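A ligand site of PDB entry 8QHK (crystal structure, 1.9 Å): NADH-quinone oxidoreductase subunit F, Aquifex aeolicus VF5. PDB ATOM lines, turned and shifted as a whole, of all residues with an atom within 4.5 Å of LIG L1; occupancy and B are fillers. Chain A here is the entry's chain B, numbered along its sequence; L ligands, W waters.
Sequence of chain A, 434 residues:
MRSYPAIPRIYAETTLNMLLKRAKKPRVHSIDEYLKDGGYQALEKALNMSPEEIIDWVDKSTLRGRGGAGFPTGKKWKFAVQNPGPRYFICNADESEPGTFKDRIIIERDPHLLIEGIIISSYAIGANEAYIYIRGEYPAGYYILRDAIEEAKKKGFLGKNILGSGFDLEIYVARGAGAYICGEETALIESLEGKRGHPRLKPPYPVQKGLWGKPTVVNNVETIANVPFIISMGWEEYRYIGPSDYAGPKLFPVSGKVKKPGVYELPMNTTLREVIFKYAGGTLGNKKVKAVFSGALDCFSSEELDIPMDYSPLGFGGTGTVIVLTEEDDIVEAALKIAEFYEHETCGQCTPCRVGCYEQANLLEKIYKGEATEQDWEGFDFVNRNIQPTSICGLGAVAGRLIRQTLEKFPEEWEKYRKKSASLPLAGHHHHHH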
ATOM      1  N   GLY A  67      22.202  -1.220   6.650  1.00  0.00           N
ATOM      2  CA  GLY A  67      21.287  -2.345   6.569  1.00  0.00           C
ATOM      3  C   GLY A  67      21.974  -3.604   6.024  1.00  0.00           C
ATOM      4  O   GLY A  67      21.394  -4.692   6.123  1.00  0.00           O
ATOM      5  N   GLY A  68      23.150  -3.439   5.415  1.00  0.00           N
ATOM      6  CA  GLY A  68      23.948  -4.593   5.015  1.00  0.00           C
ATOM      7  C   GLY A  68      24.678  -4.462   3.672  1.00  0.00           C
ATOM      8  O   GLY A  68      25.708  -5.094   3.496  1.00  0.00           O
ATOM      9  N   ALA A  69      24.131  -3.679   2.720  1.00  0.00           N
ATOM     10  CA  ALA A  69      24.693  -3.601   1.375  1.00  0.00           C
ATOM     11  C   ALA A  69      25.686  -2.463   1.220  1.00  0.00           C
ATOM     12  O   ALA A  69      26.397  -2.402   0.216  1.00  0.00           O
ATOM     13  CB  ALA A  69      23.593  -3.455   0.352  1.00  0.00           C
ATOM     14  N   PHE A  71      25.312   0.747   0.425  1.00  0.00           N
ATOM     15  CA  PHE A  71      25.117   1.729  -0.629  1.00  0.00           C
ATOM     16  C   PHE A  71      25.299   3.145  -0.068  1.00  0.00           C
ATOM     17  O   PHE A  71      24.785   3.484   0.990  1.00  0.00           O
ATOM     18  CB  PHE A  71      23.767   1.536  -1.320  1.00  0.00           C
ATOM     19  CG  PHE A  71      23.626   2.313  -2.598  1.00  0.00           C
ATOM     20  CD1 PHE A  71      23.206   3.640  -2.579  1.00  0.00           C
ATOM     21  CD2 PHE A  71      23.964   1.752  -3.824  1.00  0.00           C
ATOM     22  CE1 PHE A  71      23.080   4.366  -3.759  1.00  0.00           C
ATOM     23  CE2 PHE A  71      23.854   2.480  -4.998  1.00  0.00           C
ATOM     24  CZ  PHE A  71      23.413   3.786  -4.965  1.00  0.00           C
ATOM     25  N   LYS A  76      22.083   7.801  -2.763  1.00  0.00           N
ATOM     26  CA  LYS A  76      20.726   7.294  -2.883  1.00  0.00           C
ATOM     27  C   LYS A  76      19.729   8.457  -2.868  1.00  0.00           C
ATOM     28  O   LYS A  76      18.821   8.508  -3.692  1.00  0.00           O
ATOM     29  CB  LYS A  76      20.421   6.314  -1.748  1.00  0.00           C
ATOM     30  CG  LYS A  76      19.122   5.516  -1.932  1.00  0.00           C
ATOM     31  CD  LYS A  76      18.706   4.720  -0.714  1.00  0.00           C
ATOM     32  CE  LYS A  76      19.724   3.656  -0.323  1.00  0.00           C
ATOM     33  NZ  LYS A  76      19.172   2.714   0.672  1.00  0.00           N
ATOM     34  N   PHE A  79      19.577  10.369  -6.123  1.00  0.00           N
ATOM     35  CA  PHE A  79      18.818   9.658  -7.146  1.00  0.00           C
ATOM     36  C   PHE A  79      17.327   9.903  -6.952  1.00  0.00           C
ATOM     37  O   PHE A  79      16.593  10.078  -7.925  1.00  0.00           O
ATOM     38  CB  PHE A  79      19.122   8.151  -7.142  1.00  0.00           C
ATOM     39  CG  PHE A  79      20.358   7.718  -7.899  1.00  0.00           C
ATOM     40  CD1 PHE A  79      20.426   7.851  -9.282  1.00  0.00           C
ATOM     41  CD2 PHE A  79      21.447   7.181  -7.229  1.00  0.00           C
ATOM     42  CE1 PHE A  79      21.554   7.446  -9.984  1.00  0.00           C
ATOM     43  CE2 PHE A  79      22.575   6.776  -7.931  1.00  0.00           C
ATOM     44  CZ  PHE A  79      22.622   6.911  -9.308  1.00  0.00           C
ATOM     45  N   GLU A  95      14.624  -5.589  10.811  1.00  0.00           N
ATOM     46  CA  GLU A  95      15.751  -6.364  11.333  1.00  0.00           C
ATOM     47  C   GLU A  95      15.386  -7.791  11.763  1.00  0.00           C
ATOM     48  O   GLU A  95      14.903  -8.005  12.880  1.00  0.00           O
ATOM     49  CB  GLU A  95      16.374  -5.609  12.508  1.00  0.00           C
ATOM     50  CG  GLU A  95      17.524  -6.354  13.177  1.00  0.00           C
ATOM     51  CD  GLU A  95      18.173  -5.540  14.286  1.00  0.00           C
ATOM     52  OE1 GLU A  95      17.492  -5.308  15.320  1.00  0.00           O
ATOM     53  OE2 GLU A  95      19.342  -5.105  14.078  1.00  0.00           O
ATOM     54  N   SER A  96      15.652  -8.762  10.884  1.00  0.00           N
ATOM     55  CA  SER A  96      15.298 -10.160  11.114  1.00  0.00           C
ATOM     56  C   SER A  96      16.421 -11.117  10.723  1.00  0.00           C
ATOM     57  O   SER A  96      16.217 -12.328  10.797  1.00  0.00           O
ATOM     58  CB  SER A  96      14.040 -10.505  10.344  1.00  0.00           C
ATOM     59  OG  SER A  96      12.908  -9.866  10.918  1.00  0.00           O
ATOM     60  N   GLU A  97      17.583 -10.593  10.296  1.00  0.00           N
ATOM     61  CA  GLU A  97      18.731 -11.424   9.963  1.00  0.00           C
ATOM     62  C   GLU A  97      19.240 -12.135  11.215  1.00  0.00           C
ATOM     63  O   GLU A  97      19.466 -11.509  12.244  1.00  0.00           O
ATOM     64  CB  GLU A  97      19.881 -10.562   9.427  1.00  0.00           C
ATOM     65  CG  GLU A  97      21.100 -11.349   8.957  1.00  0.00           C
ATOM     66  CD  GLU A  97      20.955 -12.028   7.610  1.00  0.00           C
ATOM     67  OE1 GLU A  97      19.801 -12.158   7.140  1.00  0.00           O
ATOM     68  OE2 GLU A  97      21.998 -12.409   7.016  1.00  0.00           O
ATOM     69  N   THR A 100      21.236 -10.637  14.408  1.00  0.00           N
ATOM     70  CA  THR A 100      21.243  -9.200  14.170  1.00  0.00           C
ATOM     71  C   THR A 100      20.237  -8.520  15.095  1.00  0.00           C
ATOM     72  O   THR A 100      19.030  -8.760  15.027  1.00  0.00           O
ATOM     73  CB  THR A 100      21.042  -8.886  12.678  1.00  0.00           C
ATOM     74  OG1 THR A 100      21.967  -9.682  11.918  1.00  0.00           O
ATOM     75  CG2 THR A 100      21.257  -7.424  12.356  1.00  0.00           C
ATOM     76  N   TYR A 180      10.510 -12.440   7.074  1.00  0.00           N
ATOM     77  CA  TYR A 180      11.865 -11.927   6.867  1.00  0.00           C
ATOM     78  C   TYR A 180      11.989 -11.142   5.569  1.00  0.00           C
ATOM     79  O   TYR A 180      12.753 -10.170   5.495  1.00  0.00           O
ATOM     80  CB  TYR A 180      12.801 -13.128   6.796  1.00  0.00           C
ATOM     81  CG  TYR A 180      14.226 -12.934   6.322  1.00  0.00           C
ATOM     82  CD1 TYR A 180      15.184 -12.337   7.124  1.00  0.00           C
ATOM     83  CD2 TYR A 180      14.634 -13.471   5.120  1.00  0.00           C
ATOM     84  CE1 TYR A 180      16.510 -12.239   6.718  1.00  0.00           C
ATOM     85  CE2 TYR A 180      15.950 -13.379   4.695  1.00  0.00           C
ATOM     86  CZ  TYR A 180      16.889 -12.770   5.493  1.00  0.00           C
ATOM     87  OH  TYR A 180      18.197 -12.721   5.054  1.00  0.00           O
ATOM     88  N   GLU A 185      13.577  -4.192   0.490  1.00  0.00           N
ATOM     89  CA  GLU A 185      12.966  -2.866   0.439  1.00  0.00           C
ATOM     90  C   GLU A 185      11.695  -2.861  -0.420  1.00  0.00           C
ATOM     91  O   GLU A 185      10.770  -2.117  -0.103  1.00  0.00           O
ATOM     92  CB  GLU A 185      13.971  -1.827  -0.051  1.00  0.00           C
ATOM     93  CG  GLU A 185      14.536  -2.114  -1.427  1.00  0.00           C
ATOM     94  CD  GLU A 185      15.562  -1.121  -1.925  1.00  0.00           C
ATOM     95  OE1 GLU A 185      15.829  -0.135  -1.199  1.00  0.00           O
ATOM     96  OE2 GLU A 185      16.079  -1.340  -3.037  1.00  0.00           O
ATOM     97  N   TYR A 205      14.621   0.941  -9.047  1.00  0.00           N
ATOM     98  CA  TYR A 205      14.865   1.048  -7.618  1.00  0.00           C
ATOM     99  C   TYR A 205      13.784   1.929  -7.005  1.00  0.00           C
ATOM    100  O   TYR A 205      13.116   2.704  -7.709  1.00  0.00           O
ATOM    101  CB  TYR A 205      16.310   1.534  -7.370  1.00  0.00           C
ATOM    102  CG  TYR A 205      17.347   0.502  -7.759  1.00  0.00           C
ATOM    103  CD1 TYR A 205      17.690  -0.528  -6.899  1.00  0.00           C
ATOM    104  CD2 TYR A 205      17.906   0.502  -9.030  1.00  0.00           C
ATOM    105  CE1 TYR A 205      18.588  -1.508  -7.271  1.00  0.00           C
ATOM    106  CE2 TYR A 205      18.820  -0.473  -9.413  1.00  0.00           C
ATOM    107  CZ  TYR A 205      19.168  -1.470  -8.528  1.00  0.00           C
ATOM    108  OH  TYR A 205      20.074  -2.447  -8.906  1.00  0.00           O
ATOM    109  N   PRO A 206      13.535   1.801  -5.672  1.00  0.00           N
ATOM    110  CA  PRO A 206      12.493   2.578  -5.006  1.00  0.00           C
ATOM    111  C   PRO A 206      12.628   4.079  -5.265  1.00  0.00           C
ATOM    112  O   PRO A 206      11.603   4.758  -5.385  1.00  0.00           O
ATOM    113  CB  PRO A 206      12.695   2.221  -3.517  1.00  0.00           C
ATOM    114  CG  PRO A 206      13.250   0.815  -3.570  1.00  0.00           C
ATOM    115  CD  PRO A 206      14.195   0.856  -4.753  1.00  0.00           C
ATOM    116  N   VAL A 207      13.870   4.565  -5.391  1.00  0.00           N
ATOM    117  CA  VAL A 207      14.143   5.979  -5.550  1.00  0.00           C
ATOM    118  C   VAL A 207      13.555   6.496  -6.863  1.00  0.00           C
ATOM    119  O   VAL A 207      13.248   7.690  -6.959  1.00  0.00           O
ATOM    120  CB  VAL A 207      15.637   6.324  -5.444  1.00  0.00           C
ATOM    121  CG1 VAL A 207      16.126   6.147  -4.013  1.00  0.00           C
ATOM    122  CG2 VAL A 207      16.491   5.539  -6.427  1.00  0.00           C
ATOM    123  N   VAL A 218      14.360   4.128   0.940  1.00  0.00           N
ATOM    124  CA  VAL A 218      14.393   3.213   2.060  1.00  0.00           C
ATOM    125  C   VAL A 218      15.794   3.263   2.669  1.00  0.00           C
ATOM    126  O   VAL A 218      16.782   3.120   1.946  1.00  0.00           O
ATOM    127  CB  VAL A 218      14.021   1.769   1.665  1.00  0.00           C
ATOM    128  CG1 VAL A 218      13.956   0.863   2.884  1.00  0.00           C
ATOM    129  CG2 VAL A 218      12.725   1.720   0.878  1.00  0.00           C
ATOM    130  N   LEU A 297      24.796 -14.655   5.887  1.00  0.00           N
ATOM    131  CA  LEU A 297      25.329 -14.180   4.625  1.00  0.00           C
ATOM    132  C   LEU A 297      26.696 -14.823   4.321  1.00  0.00           C
ATOM    133  O   LEU A 297      26.873 -15.388   3.242  1.00  0.00           O
ATOM    134  CB  LEU A 297      25.412 -12.650   4.682  1.00  0.00           C
ATOM    135  CG  LEU A 297      25.998 -11.945   3.457  1.00  0.00           C
ATOM    136  CD1 LEU A 297      25.080 -12.090   2.239  1.00  0.00           C
ATOM    137  CD2 LEU A 297      26.255 -10.477   3.760  1.00  0.00           C
ATOM    138  N   GLY A 318      28.609  -6.634   5.292  1.00  0.00           N
ATOM    139  CA  GLY A 318      27.296  -7.021   5.775  1.00  0.00           C
ATOM    140  C   GLY A 318      26.754  -6.043   6.819  1.00  0.00           C
ATOM    141  O   GLY A 318      26.934  -4.833   6.726  1.00  0.00           O
ATOM    142  N   THR A 319      26.034  -6.612   7.801  1.00  0.00           N
ATOM    143  CA  THR A 319      25.389  -5.861   8.866  1.00  0.00           C
ATOM    144  C   THR A 319      26.364  -5.570  10.012  1.00  0.00           C
ATOM    145  O   THR A 319      26.047  -4.785  10.897  1.00  0.00           O
ATOM    146  CB  THR A 319      24.184  -6.641   9.374  1.00  0.00           C
ATOM    147  OG1 THR A 319      24.628  -7.946   9.747  1.00  0.00           O
ATOM    148  CG2 THR A 319      23.072  -6.782   8.352  1.00  0.00           C
ATOM    149  N   GLY A 394      17.669 -10.444  -3.257  1.00  0.00           N
ATOM    150  CA  GLY A 394      18.930 -10.850  -2.659  1.00  0.00           C
ATOM    151  C   GLY A 394      18.848 -12.159  -1.865  1.00  0.00           C
ATOM    152  O   GLY A 394      19.883 -12.762  -1.579  1.00  0.00           O
HETATM  153  O1  LIG L   1      17.784  -7.834   9.100  1.00  0.00           O
HETATM  154  C1  LIG L   1      18.584  -7.276   8.352  1.00  0.00           C
HETATM  155  C2  LIG L   1      19.261  -6.014   8.775  1.00  0.00           C
HETATM  156  C3  LIG L   1      18.850  -7.860   7.021  1.00  0.00           C
HETATM  157  C4  LIG L   1      18.087  -9.093   6.631  1.00  0.00           C
HETATM  158  C5  LIG L   1      18.480  -9.593   5.288  1.00  0.00           C
HETATM  159  C6  LIG L   1      19.406  -8.999   4.545  1.00  0.00           C
HETATM  160  C7  LIG L   1      19.751  -7.305   6.182  1.00  0.00           C
HETATM  161  N1  LIG L   1      20.055  -7.855   4.945  1.00  0.00           N
HETATM  162  C8  LIG L   1      21.060  -7.260   4.075  1.00  0.00           C
HETATM  163  C9  LIG L   1      22.249  -8.166   3.754  1.00  0.00           C
HETATM  164  O2  LIG L   1      23.398  -7.853   4.550  1.00  0.00           O
HETATM  165  C10 LIG L   1      22.549  -7.877   2.270  1.00  0.00           C
HETATM  166  O3  LIG L   1      23.854  -7.341   2.131  1.00  0.00           O
HETATM  167  O4  LIG L   1      20.456  -6.941   2.838  1.00  0.00           O
HETATM  168  C11 LIG L   1      21.536  -6.801   1.893  1.00  0.00           C
HETATM  169  C12 LIG L   1      21.009  -6.881   0.474  1.00  0.00           C
HETATM  170  O5  LIG L   1      20.153  -5.739   0.260  1.00  0.00           O
HETATM  171  P1  LIG L   1      19.666  -5.304  -1.182  1.00  0.00           P
HETATM  172  O6  LIG L   1      19.268  -6.505  -1.944  1.00  0.00           O
HETATM  173  O7  LIG L   1      18.689  -4.214  -0.938  1.00  0.00           O
HETATM  174  O8  LIG L   1      21.028  -4.703  -1.795  1.00  0.00           O
HETATM  175  P2  LIG L   1      21.396  -3.846  -3.080  1.00  0.00           P
HETATM  176  O9  LIG L   1      20.647  -4.322  -4.265  1.00  0.00           O
HETATM  177  O10 LIG L   1      22.867  -3.799  -3.169  1.00  0.00           O
HETATM  178  O11 LIG L   1      20.826  -2.388  -2.718  1.00  0.00           O
HETATM  179  C13 LIG L   1      21.253  -1.653  -1.553  1.00  0.00           C
HETATM  180  C14 LIG L   1      20.539  -0.332  -1.519  1.00  0.00           C
HETATM  181  O12 LIG L   1      21.088   0.540  -2.532  1.00  0.00           O
HETATM  182  C15 LIG L   1      20.078   0.905  -3.466  1.00  0.00           C
HETATM  183  C16 LIG L   1      18.936  -0.103  -3.291  1.00  0.00           C
HETATM  184  O13 LIG L   1      17.677   0.432  -3.672  1.00  0.00           O
HETATM  185  C17 LIG L   1      19.023  -0.381  -1.790  1.00  0.00           C
HETATM  186  O14 LIG L   1      18.351   0.646  -1.081  1.00  0.00           O
HETATM  187  N2  LIG L   1      20.667   0.891  -4.792  1.00  0.00           N
HETATM  188  C18 LIG L   1      21.470  -0.084  -5.330  1.00  0.00           C
HETATM  189  N3  LIG L   1      21.772   0.099  -6.592  1.00  0.00           N
HETATM  190  C19 LIG L   1      21.112   1.277  -6.924  1.00  0.00           C
HETATM  191  C20 LIG L   1      21.011   2.010  -8.120  1.00  0.00           C
HETATM  192  N4  LIG L   1      21.553   1.613  -9.275  1.00  0.00           N
HETATM  193  C21 LIG L   1      20.430   1.774  -5.824  1.00  0.00           C
HETATM  194  N5  LIG L   1      19.697   2.893  -5.780  1.00  0.00           N
HETATM  195  C22 LIG L   1      19.672   3.501  -6.974  1.00  0.00           C
HETATM  196  N6  LIG L   1      20.278   3.135  -8.110  1.00  0.00           N
HETATM  197  C1  LG2 L   2      17.102  -6.807   3.240  1.00  0.00           C
HETATM  198  N1  LG2 L   2      17.513  -5.514   3.703  1.00  0.00           N
HETATM  199  C2  LG2 L   2      17.140  -5.121   4.968  1.00  0.00           C
HETATM  200  N2  LG2 L   2      17.485  -3.861   5.387  1.00  0.00           N
HETATM  201  C3  LG2 L   2      17.154  -3.365   6.613  1.00  0.00           C
HETATM  202  O1  LG2 L   2      17.393  -2.203   6.936  1.00  0.00           O
HETATM  203  N3  LG2 L   2      16.454  -4.217   7.438  1.00  0.00           N
HETATM  204  C4  LG2 L   2      16.028  -5.504   7.130  1.00  0.00           C
HETATM  205  O2  LG2 L   2      15.382  -6.143   7.965  1.00  0.00           O
HETATM  206  C5  LG2 L   2      16.389  -5.927   5.812  1.00  0.00           C
HETATM  207  N4  LG2 L   2      15.971  -7.135   5.359  1.00  0.00           N
HETATM  208  C6  LG2 L   2      16.293  -7.587   4.082  1.00  0.00           C
HETATM  209  C7  LG2 L   2      15.851  -8.844   3.666  1.00  0.00           C
HETATM  210  C8  LG2 L   2      16.212  -9.339   2.429  1.00  0.00           C
HETATM  211  C9  LG2 L   2      15.742 -10.717   2.009  1.00  0.00           C
HETATM  212  C10 LG2 L   2      17.040  -8.568   1.575  1.00  0.00           C
HETATM  213  C11 LG2 L   2      17.522  -9.114   0.256  1.00  0.00           C
HETATM  214  C12 LG2 L   2      17.468  -7.307   1.991  1.00  0.00           C
HETATM  215  C13 LG2 L   2      18.216  -4.583   2.804  1.00  0.00           C
HETATM  216  C14 LG2 L   2      17.193  -3.630   2.164  1.00  0.00           C
HETATM  217  O3  LG2 L   2      16.685  -4.252   0.981  1.00  0.00           O
HETATM  218  C15 LG2 L   2      17.865  -2.297   1.807  1.00  0.00           C
HETATM  219  O4  LG2 L   2      19.117  -2.506   1.161  1.00  0.00           O
HETATM  220  C16 LG2 L   2      18.097  -1.354   2.993  1.00  0.00           C
HETATM  221  O5  LG2 L   2      16.951  -1.250   3.851  1.00  0.00           O
HETATM  222  C17 LG2 L   2      18.508   0.018   2.513  1.00  0.00           C
HETATM  223  O6  LG2 L   2      18.908   0.829   3.633  1.00  0.00           O
HETATM  224  P1  LG2 L   2      20.479   1.230   3.828  1.00  0.00           P
HETATM  225  O7  LG2 L   2      20.963   1.726   2.481  1.00  0.00           O
HETATM  226  O8  LG2 L   2      20.420   2.342   4.868  1.00  0.00           O
HETATM  227  O9  LG2 L   2      21.180  -0.017   4.307  1.00  0.00           O
HETATM  228  O   HOH W   1      24.571  -1.799  -4.318  1.00  0.00           O
HETATM  229  O   HOH W   2      24.792  -7.075  -0.339  1.00  0.00           O
HETATM  230  O   HOH W   3      20.979  -8.258  -2.917  1.00  0.00           O
HETATM  231  O   HOH W   4      17.088  -7.415  -3.081  1.00  0.00           O
HETATM  232  O   HOH W   5      19.917  -4.562  11.362  1.00  0.00           O
HETATM  233  O   HOH W   6      19.792   4.245 -10.481  1.00  0.00           O
HETATM  234  O   HOH W   7      24.472  -5.767  -2.375  1.00  0.00           O
HETATM  235  O   HOH W   8      23.439  -9.896   6.364  1.00  0.00           O
HETATM  236  O   HOH W   9      16.928  -3.896  -3.338  1.00  0.00           O
HETATM  237  O   HOH W  10      17.041   3.028  -4.034  1.00  0.00           O
HETATM  238  O   HOH W  11      22.900  -1.035  -9.645  1.00  0.00           O
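N of Glu 185 lies within hydrogen-bond range of O3 of LG2 L2 (3.1 Å).
The side-chain carboxylate of Glu 185 is in hydrogen-bond range of an oxygen (O13) of LIG L1 (2.5 Å).
An oxygen (O14) of LIG L1 is in hydrogen-bond range of the side-chain amino group (NZ) of Lys 76 (2.8 Å).
An oxygen (O7) of LG2 L2 is in salt-bridge range of the side-chain amino group (NZ) of Lys 76 (2.7 Å).
The backbone NH (N) of Glu 95 is in hydrogen-bond range of an oxygen (O2) of LG2 L2, at 3.0 Å.
An oxygen (O1) of LIG L1 is in hydrogen-bond range of the backbone NH (N) of Glu 97, at 3.0 Å.
O3 of LIG L1 lies within hydrogen-bond range of O of Gly 68 (3.2 Å).
N of Ser 96 sits at hydrogen-bond distance from O1 of LIG L1.
O9 of LG2 L2 sits at hydrogen-bond distance from N of Gly 67, at 2.8 Å.
O7 of LIG L1 sits at hydrogen-bond distance from O4 of LG2 L2 (2.7 Å).
OH of Tyr 180 lies within hydrogen-bond range of OE1 of Glu 97, 2.7 Å away.
O of Glu 97 sits close to OG1 of Thr 100, 3.1 Å away.
The side-chain amino group (NZ) of Lys 76 lies within hydrogen-bond range of the backbone carbonyl oxygen (O) of Val 218 (2.7 Å).
Merely in contact with LIG L1: Gly 67 (3.1 Å), Ala 69 (3.5 Å), Phe 71 (3.1 Å), Glu 95 (3.4 Å), Tyr 180 (3.1 Å), Tyr 205 (3.4 Å), Pro 206 (3.7 Å), Val 207 (3.8 Å), Leu 297 (3.96 Å) and Thr 319 (3.9 Å).
Water W4 lies within hydrogen-bond range of an oxygen (O6) of LIG L1 and the backbone NH (N) of Gly 394.
Water W8 bridges an oxygen (O2) of LIG L1 (2.7 Å) and the side-chain carboxylate of Glu 97 (3.0 Å).
Water W9 bridges OE2 of Glu 185 (2.7 Å) and O7 of LIG L1 (3.0 Å).
Water W11 lies within hydrogen-bond range of a nitrogen (N4) of LIG L1 (3.0 Å) and the side-chain hydroxyl (OH) of Tyr 205 (3.2 Å).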
